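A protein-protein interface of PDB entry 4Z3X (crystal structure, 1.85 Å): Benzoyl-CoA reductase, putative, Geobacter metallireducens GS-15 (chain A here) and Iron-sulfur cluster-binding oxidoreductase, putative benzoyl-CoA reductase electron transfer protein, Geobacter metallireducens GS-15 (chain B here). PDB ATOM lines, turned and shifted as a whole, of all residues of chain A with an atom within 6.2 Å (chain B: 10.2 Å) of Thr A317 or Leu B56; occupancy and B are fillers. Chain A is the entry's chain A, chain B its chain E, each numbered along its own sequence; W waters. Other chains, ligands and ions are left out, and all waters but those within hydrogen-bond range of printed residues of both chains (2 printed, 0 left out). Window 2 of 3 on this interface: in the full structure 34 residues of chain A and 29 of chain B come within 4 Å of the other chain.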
ATOM      1  N   ILE A 144     -14.591  -5.585 -17.402  1.00  0.00           N
ATOM      2  CA  ILE A 144     -14.031  -4.462 -18.165  1.00  0.00           C
ATOM      3  C   ILE A 144     -14.147  -3.162 -17.355  1.00  0.00           C
ATOM      4  O   ILE A 144     -13.208  -2.388 -17.273  1.00  0.00           O
ATOM      5  CB  ILE A 144     -14.721  -4.300 -19.573  1.00  0.00           C
ATOM      6  CG1 ILE A 144     -14.416  -5.524 -20.428  1.00  0.00           C
ATOM      7  CG2 ILE A 144     -14.228  -3.048 -20.301  1.00  0.00           C
ATOM      8  CD1 ILE A 144     -12.909  -5.748 -20.622  1.00  0.00           C
ATOM      9  N   GLU A 148     -11.192  -0.356 -16.127  1.00  0.00           N
ATOM     10  CA  GLU A 148     -11.170   1.090 -16.432  1.00  0.00           C
ATOM     11  C   GLU A 148     -11.061   1.896 -15.151  1.00  0.00           C
ATOM     12  O   GLU A 148     -10.328   2.871 -15.094  1.00  0.00           O
ATOM     13  CB  GLU A 148     -12.422   1.490 -17.225  1.00  0.00           C
ATOM     14  CG  GLU A 148     -12.475   0.851 -18.655  1.00  0.00           C
ATOM     15  CD  GLU A 148     -11.172   1.117 -19.434  1.00  0.00           C
ATOM     16  OE1 GLU A 148     -10.755   2.297 -19.488  1.00  0.00           O
ATOM     17  OE2 GLU A 148     -10.529   0.167 -19.948  1.00  0.00           O
ATOM     18  N   THR A 294     -18.426  -2.040 -34.420  1.00  0.00           N
ATOM     19  CA  THR A 294     -17.773  -0.730 -34.488  1.00  0.00           C
ATOM     20  C   THR A 294     -16.468  -0.777 -35.280  1.00  0.00           C
ATOM     21  O   THR A 294     -16.268   0.017 -36.193  1.00  0.00           O
ATOM     22  CB  THR A 294     -17.500  -0.192 -33.080  1.00  0.00           C
ATOM     23  OG1 THR A 294     -18.746  -0.088 -32.378  1.00  0.00           O
ATOM     24  CG2 THR A 294     -16.789   1.161 -33.135  1.00  0.00           C
ATOM     25  N   THR A 309     -15.071  -4.630 -31.669  1.00  0.00           N
ATOM     26  CA  THR A 309     -15.829  -3.902 -30.677  1.00  0.00           C
ATOM     27  C   THR A 309     -17.302  -3.997 -31.099  1.00  0.00           C
ATOM     28  O   THR A 309     -17.631  -3.888 -32.276  1.00  0.00           O
ATOM     29  CB  THR A 309     -15.367  -2.392 -30.558  1.00  0.00           C
ATOM     30  OG1 THR A 309     -14.935  -1.941 -31.828  1.00  0.00           O
ATOM     31  CG2 THR A 309     -14.208  -2.281 -29.633  1.00  0.00           C
ATOM     32  N   ILE A 310     -18.173  -4.180 -30.123  1.00  0.00           N
ATOM     33  CA  ILE A 310     -19.574  -4.414 -30.381  1.00  0.00           C
ATOM     34  C   ILE A 310     -20.379  -3.448 -29.559  1.00  0.00           C
ATOM     35  O   ILE A 310     -20.285  -3.417 -28.323  1.00  0.00           O
ATOM     36  CB  ILE A 310     -20.007  -5.858 -30.001  1.00  0.00           C
ATOM     37  CG1 ILE A 310     -19.304  -6.881 -30.880  1.00  0.00           C
ATOM     38  CG2 ILE A 310     -21.535  -6.010 -30.115  1.00  0.00           C
ATOM     39  CD1 ILE A 310     -19.788  -6.828 -32.365  1.00  0.00           C
ATOM     40  N   SER A 311     -21.226  -2.710 -30.241  1.00  0.00           N
ATOM     41  CA  SER A 311     -21.970  -1.685 -29.577  1.00  0.00           C
ATOM     42  C   SER A 311     -23.460  -1.846 -29.815  1.00  0.00           C
ATOM     43  O   SER A 311     -23.952  -1.588 -30.899  1.00  0.00           O
ATOM     44  CB  SER A 311     -21.475  -0.311 -30.048  1.00  0.00           C
ATOM     45  OG  SER A 311     -22.329   0.691 -29.550  1.00  0.00           O
ATOM     46  N   MET A 312     -24.180  -2.291 -28.795  1.00  0.00           N
ATOM     47  CA  MET A 312     -25.633  -2.453 -28.866  1.00  0.00           C
ATOM     48  C   MET A 312     -26.302  -1.239 -28.248  1.00  0.00           C
ATOM     49  O   MET A 312     -25.833  -0.736 -27.229  1.00  0.00           O
ATOM     50  CB  MET A 312     -26.095  -3.736 -28.140  1.00  0.00           C
ATOM     51  CG  MET A 312     -25.476  -5.013 -28.681  1.00  0.00           C
ATOM     52  SD  MET A 312     -25.694  -5.228 -30.464  1.00  0.00           S
ATOM     53  CE  MET A 312     -27.481  -5.462 -30.525  1.00  0.00           C
ATOM     54  N   LEU A 315     -26.388  -0.144 -24.395  1.00  0.00           N
ATOM     55  CA  LEU A 315     -25.526  -1.045 -23.641  1.00  0.00           C
ATOM     56  C   LEU A 315     -24.087  -0.582 -23.764  1.00  0.00           C
ATOM     57  O   LEU A 315     -23.713   0.017 -24.749  1.00  0.00           O
ATOM     58  CB  LEU A 315     -25.674  -2.511 -24.121  1.00  0.00           C
ATOM     59  CG  LEU A 315     -26.953  -3.307 -23.825  1.00  0.00           C
ATOM     60  CD1 LEU A 315     -26.933  -4.693 -24.499  1.00  0.00           C
ATOM     61  CD2 LEU A 315     -27.203  -3.457 -22.336  1.00  0.00           C
ATOM     62  N   PRO A 316     -23.263  -0.870 -22.750  1.00  0.00           N
ATOM     63  CA  PRO A 316     -21.864  -0.457 -22.850  1.00  0.00           C
ATOM     64  C   PRO A 316     -21.191  -1.209 -23.977  1.00  0.00           C
ATOM     65  O   PRO A 316     -21.631  -2.312 -24.315  1.00  0.00           O
ATOM     66  CB  PRO A 316     -21.272  -0.841 -21.472  1.00  0.00           C
ATOM     67  CG  PRO A 316     -22.476  -1.019 -20.586  1.00  0.00           C
ATOM     68  CD  PRO A 316     -23.562  -1.523 -21.465  1.00  0.00           C
ATOM     69  N   THR A 317     -20.151  -0.634 -24.562  1.00  0.00           N
ATOM     70  CA  THR A 317     -19.389  -1.348 -25.563  1.00  0.00           C
ATOM     71  C   THR A 317     -18.684  -2.578 -24.969  1.00  0.00           C
ATOM     72  O   THR A 317     -18.180  -2.533 -23.845  1.00  0.00           O
ATOM     73  CB  THR A 317     -18.384  -0.423 -26.206  1.00  0.00           C
ATOM     74  OG1 THR A 317     -19.103   0.507 -27.038  1.00  0.00           O
ATOM     75  CG2 THR A 317     -17.391  -1.182 -27.063  1.00  0.00           C
ATOM     76  N   TYR A 318     -18.654  -3.688 -25.707  1.00  0.00           N
ATOM     77  CA  TYR A 318     -17.749  -4.790 -25.325  1.00  0.00           C
ATOM     78  C   TYR A 318     -17.037  -5.360 -26.565  1.00  0.00           C
ATOM     79  O   TYR A 318     -17.220  -4.876 -27.696  1.00  0.00           O
ATOM     80  CB  TYR A 318     -18.490  -5.887 -24.572  1.00  0.00           C
ATOM     81  CG  TYR A 318     -19.433  -6.707 -25.426  1.00  0.00           C
ATOM     82  CD1 TYR A 318     -20.611  -6.153 -25.916  1.00  0.00           C
ATOM     83  CD2 TYR A 318     -19.167  -8.042 -25.699  1.00  0.00           C
ATOM     84  CE1 TYR A 318     -21.490  -6.885 -26.690  1.00  0.00           C
ATOM     85  CE2 TYR A 318     -20.047  -8.803 -26.470  1.00  0.00           C
ATOM     86  CZ  TYR A 318     -21.208  -8.212 -26.957  1.00  0.00           C
ATOM     87  OH  TYR A 318     -22.088  -8.944 -27.705  1.00  0.00           O
ATOM     88  N   MET A 319     -16.205  -6.371 -26.336  1.00  0.00           N
ATOM     89  CA  MET A 319     -15.395  -6.953 -27.398  1.00  0.00           C
ATOM     90  C   MET A 319     -15.684  -8.441 -27.563  1.00  0.00           C
ATOM     91  O   MET A 319     -15.913  -9.174 -26.576  1.00  0.00           O
ATOM     92  CB  MET A 319     -13.922  -6.692 -27.124  1.00  0.00           C
ATOM     93  CG  MET A 319     -13.563  -5.212 -27.508  1.00  0.00           C
ATOM     94  SD  MET A 319     -12.490  -4.286 -26.436  1.00  0.00           S
ATOM     95  CE  MET A 319     -13.446  -4.272 -24.926  1.00  0.00           C
ATOM     96  N   GLN A 344     -23.090  -9.275 -23.987  1.00  0.00           N
ATOM     97  CA  GLN A 344     -22.513  -8.125 -23.283  1.00  0.00           C
ATOM     98  C   GLN A 344     -22.572  -8.348 -21.767  1.00  0.00           C
ATOM     99  O   GLN A 344     -21.549  -8.233 -21.079  1.00  0.00           O
ATOM    100  CB  GLN A 344     -23.247  -6.828 -23.645  1.00  0.00           C
ATOM    101  CG  GLN A 344     -22.600  -5.568 -23.101  1.00  0.00           C
ATOM    102  CD  GLN A 344     -23.022  -5.208 -21.676  1.00  0.00           C
ATOM    103  OE1 GLN A 344     -24.171  -5.343 -21.297  1.00  0.00           O
ATOM    104  NE2 GLN A 344     -22.089  -4.725 -20.907  1.00  0.00           N
ATOM    105  N   VAL B  52      -2.187   6.021 -29.768  1.00  0.00           N
ATOM    106  CA  VAL B  52      -3.250   6.310 -28.816  1.00  0.00           C
ATOM    107  C   VAL B  52      -4.348   5.279 -28.991  1.00  0.00           C
ATOM    108  O   VAL B  52      -4.997   5.251 -30.024  1.00  0.00           O
ATOM    109  CB  VAL B  52      -3.837   7.686 -29.016  1.00  0.00           C
ATOM    110  CG1 VAL B  52      -4.951   7.903 -28.013  1.00  0.00           C
ATOM    111  CG2 VAL B  52      -2.724   8.761 -28.889  1.00  0.00           C
ATOM    112  N   ARG B  53      -4.588   4.429 -27.992  1.00  0.00           N
ATOM    113  CA  ARG B  53      -5.441   3.261 -28.180  1.00  0.00           C
ATOM    114  C   ARG B  53      -6.486   3.102 -27.082  1.00  0.00           C
ATOM    115  O   ARG B  53      -6.159   2.864 -25.897  1.00  0.00           O
ATOM    116  CB  ARG B  53      -4.558   2.005 -28.267  1.00  0.00           C
ATOM    117  CG  ARG B  53      -5.319   0.737 -28.585  1.00  0.00           C
ATOM    118  CD  ARG B  53      -4.468  -0.510 -28.578  1.00  0.00           C
ATOM    119  NE  ARG B  53      -5.353  -1.628 -28.842  1.00  0.00           N
ATOM    120  CZ  ARG B  53      -6.060  -2.328 -27.942  1.00  0.00           C
ATOM    121  NH1 ARG B  53      -6.002  -2.093 -26.632  1.00  0.00           N
ATOM    122  NH2 ARG B  53      -6.860  -3.283 -28.365  1.00  0.00           N
ATOM    123  N   ASP B  54      -7.749   3.254 -27.449  1.00  0.00           N
ATOM    124  CA  ASP B  54      -8.837   3.051 -26.496  1.00  0.00           C
ATOM    125  C   ASP B  54     -10.038   2.502 -27.212  1.00  0.00           C
ATOM    126  O   ASP B  54     -10.927   3.269 -27.576  1.00  0.00           O
ATOM    127  CB  ASP B  54      -9.264   4.343 -25.737  1.00  0.00           C
ATOM    128  CG  ASP B  54     -10.246   4.042 -24.575  1.00  0.00           C
ATOM    129  OD1 ASP B  54     -10.742   2.871 -24.477  1.00  0.00           O
ATOM    130  OD2 ASP B  54     -10.482   4.941 -23.713  1.00  0.00           O
ATOM    131  N   PRO B  55     -10.147   1.154 -27.261  1.00  0.00           N
ATOM    132  CA  PRO B  55     -11.212   0.511 -28.006  1.00  0.00           C
ATOM    133  C   PRO B  55     -12.551   1.008 -27.534  1.00  0.00           C
ATOM    134  O   PRO B  55     -13.455   1.047 -28.335  1.00  0.00           O
ATOM    135  CB  PRO B  55     -11.057  -1.020 -27.658  1.00  0.00           C
ATOM    136  CG  PRO B  55      -9.824  -1.165 -26.862  1.00  0.00           C
ATOM    137  CD  PRO B  55      -9.368   0.236 -26.412  1.00  0.00           C
ATOM    138  N   LEU B  56     -12.712   1.341 -26.260  1.00  0.00           N
ATOM    139  CA  LEU B  56     -14.055   1.735 -25.769  1.00  0.00           C
ATOM    140  C   LEU B  56     -14.445   3.146 -26.212  1.00  0.00           C
ATOM    141  O   LEU B  56     -15.624   3.541 -26.173  1.00  0.00           O
ATOM    142  CB  LEU B  56     -14.112   1.624 -24.217  1.00  0.00           C
ATOM    143  CG  LEU B  56     -13.731   0.240 -23.675  1.00  0.00           C
ATOM    144  CD1 LEU B  56     -13.593   0.183 -22.075  1.00  0.00           C
ATOM    145  CD2 LEU B  56     -14.837  -0.674 -24.079  1.00  0.00           C
ATOM    146  N   ARG B  57     -13.463   3.920 -26.668  1.00  0.00           N
ATOM    147  CA  ARG B  57     -13.847   5.204 -27.288  1.00  0.00           C
ATOM    148  C   ARG B  57     -13.772   5.119 -28.796  1.00  0.00           C
ATOM    149  O   ARG B  57     -14.001   6.117 -29.462  1.00  0.00           O
ATOM    150  CB  ARG B  57     -12.963   6.340 -26.761  1.00  0.00           C
ATOM    151  CG  ARG B  57     -13.366   6.761 -25.342  1.00  0.00           C
ATOM    152  CD  ARG B  57     -12.486   7.962 -24.779  1.00  0.00           C
ATOM    153  NE  ARG B  57     -11.162   7.462 -24.405  1.00  0.00           N
ATOM    154  CZ  ARG B  57     -10.043   8.163 -24.314  1.00  0.00           C
ATOM    155  NH1 ARG B  57      -9.975   9.518 -24.529  1.00  0.00           N
ATOM    156  NH2 ARG B  57      -8.963   7.484 -23.984  1.00  0.00           N
ATOM    157  N   ASP B  58     -13.583   3.886 -29.330  1.00  0.00           N
ATOM    158  CA  ASP B  58     -13.167   3.724 -30.728  1.00  0.00           C
ATOM    159  C   ASP B  58     -12.040   4.708 -31.179  1.00  0.00           C
ATOM    160  O   ASP B  58     -12.027   5.125 -32.321  1.00  0.00           O
ATOM    161  CB  ASP B  58     -14.401   3.863 -31.662  1.00  0.00           C
ATOM    162  CG  ASP B  58     -14.107   3.482 -33.154  1.00  0.00           C
ATOM    163  OD1 ASP B  58     -13.609   2.338 -33.424  1.00  0.00           O
ATOM    164  OD2 ASP B  58     -14.414   4.318 -34.064  1.00  0.00           O
ATOM    165  N   ILE B  59     -11.052   5.003 -30.324  1.00  0.00           N
ATOM    166  CA  ILE B  59      -9.875   5.781 -30.735  1.00  0.00           C
ATOM    167  C   ILE B  59      -8.593   4.963 -31.030  1.00  0.00           C
ATOM    168  O   ILE B  59      -8.138   4.206 -30.185  1.00  0.00           O
ATOM    169  CB  ILE B  59      -9.548   6.842 -29.599  1.00  0.00           C
ATOM    170  CG1 ILE B  59     -10.722   7.782 -29.405  1.00  0.00           C
ATOM    171  CG2 ILE B  59      -8.262   7.567 -29.860  1.00  0.00           C
ATOM    172  CD1 ILE B  59     -10.493   8.802 -28.139  1.00  0.00           C
ATOM    173  N   TYR B  60      -8.028   5.094 -32.226  1.00  0.00           N
ATOM    174  CA  TYR B  60      -6.799   4.345 -32.623  1.00  0.00           C
ATOM    175  C   TYR B  60      -6.074   5.373 -33.480  1.00  0.00           C
ATOM    176  O   TYR B  60      -6.418   5.574 -34.688  1.00  0.00           O
ATOM    177  CB  TYR B  60      -7.087   3.035 -33.423  1.00  0.00           C
ATOM    178  CG  TYR B  60      -8.047   2.109 -32.739  1.00  0.00           C
ATOM    179  CD1 TYR B  60      -9.403   2.354 -32.828  1.00  0.00           C
ATOM    180  CD2 TYR B  60      -7.616   1.014 -31.961  1.00  0.00           C
ATOM    181  CE1 TYR B  60     -10.305   1.561 -32.221  1.00  0.00           C
ATOM    182  CE2 TYR B  60      -8.551   0.168 -31.343  1.00  0.00           C
ATOM    183  CZ  TYR B  60      -9.899   0.466 -31.474  1.00  0.00           C
ATOM    184  OH  TYR B  60     -10.918  -0.295 -30.909  1.00  0.00           O
ATOM    185  N   GLY B  83     -17.928  13.661 -31.505  1.00  0.00           N
ATOM    186  CA  GLY B  83     -18.443  12.853 -30.419  1.00  0.00           C
ATOM    187  C   GLY B  83     -17.400  12.066 -29.682  1.00  0.00           C
ATOM    188  O   GLY B  83     -17.719  11.368 -28.738  1.00  0.00           O
ATOM    189  N   LYS B  84     -16.148  12.136 -30.100  1.00  0.00           N
ATOM    190  CA  LYS B  84     -15.127  11.416 -29.399  1.00  0.00           C
ATOM    191  C   LYS B  84     -14.482  12.400 -28.432  1.00  0.00           C
ATOM    192  O   LYS B  84     -14.050  13.461 -28.853  1.00  0.00           O
ATOM    193  CB  LYS B  84     -14.101  10.838 -30.374  1.00  0.00           C
ATOM    194  CG  LYS B  84     -14.621   9.654 -31.225  1.00  0.00           C
ATOM    195  CD  LYS B  84     -13.533   9.148 -32.163  1.00  0.00           C
ATOM    196  CE  LYS B  84     -13.958   7.775 -32.683  1.00  0.00           C
ATOM    197  NZ  LYS B  84     -13.222   7.293 -33.866  1.00  0.00           N
ATOM    198  N   GLU B  85     -14.477  12.079 -27.142  1.00  0.00           N
ATOM    199  CA  GLU B  85     -13.629  12.804 -26.194  1.00  0.00           C
ATOM    200  C   GLU B  85     -12.170  12.302 -26.170  1.00  0.00           C
ATOM    201  O   GLU B  85     -11.851  11.280 -25.555  1.00  0.00           O
ATOM    202  CB  GLU B  85     -14.219  12.677 -24.802  1.00  0.00           C
ATOM    203  CG  GLU B  85     -15.726  12.690 -24.826  1.00  0.00           C
ATOM    204  CD  GLU B  85     -16.342  13.148 -23.523  1.00  0.00           C
ATOM    205  OE1 GLU B  85     -15.619  13.747 -22.684  1.00  0.00           O
ATOM    206  OE2 GLU B  85     -17.565  12.938 -23.358  1.00  0.00           O
HETATM  207  O   HOH W   1     -10.266   0.682 -23.141  1.00  0.00           O
HETATM  208  O   HOH W   2     -13.818   0.546 -31.365  1.00  0.00           O
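Ile A144 touches Leu B56. Leu B56 touches Glu A148 (CD1 to CG, 3.7 Å). Thr A294 touches Asp B58. CG2 of Thr A309 touches O of Pro B55, 3.7 Å away. O of Thr A317 touches CD2 of Leu B56, at 3.8 Å. Met A319 touches Pro B55. Met A319 touches Leu B56.
O of Thr A309 lies within hydrogen-bond range of N of Thr A294 (2.9 Å). OD1 of Asp B54 sits at hydrogen-bond distance from N of Leu B56 (3.1 Å). The side-chain carboxylate (OD2) of Asp B58 lies within salt-bridge range of the side-chain amino group (NZ) of Lys B84 (3.2 Å).
Water W1 lies within hydrogen-bond range of the side-chain carboxylate of Asp B54 and the side-chain carboxylate of Glu A148. Water W2 lies within hydrogen-bond range of the side-chain carboxylate of Asp B58 (2.7 Å), the side-chain hydroxyl of Thr A309 (2.8 Å), the side-chain hydroxyl of Tyr B60 (3.1 Å) and the backbone carbonyl oxygen of Pro B55 (3.1 Å).
Of the 12 printed residues of chain B, 3 touch a printed residue of chain A. Hydrophobic or aromatic side chains of chain B that line the printed part of chain A: Pro B55 and Leu B56. Hydrophobic or aromatic side chains of chain A within 4 Å of the printed part of chain B: Ile A144 and Met A319.
Printed residues of chain B within 4 Å of Ile A144: Leu B56. Of the printed residues of chain B, Thr A294 touches Asp B58 (3.4 Å). No residue of chain B comes within 4 Å of Pro A316. Thr A317 touches one residue of chain B. Printed residues of chain B within 4 Å of Met A319: Pro B55 (3.8 Å) and Leu B56 (3.9 Å). Gln A344 touches none of the printed residues of chain B. Leu B56 touches four residues of chain A. The nearest residue of chain B that does not touch Thr A317 is Pro B55 (4.7 Å).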
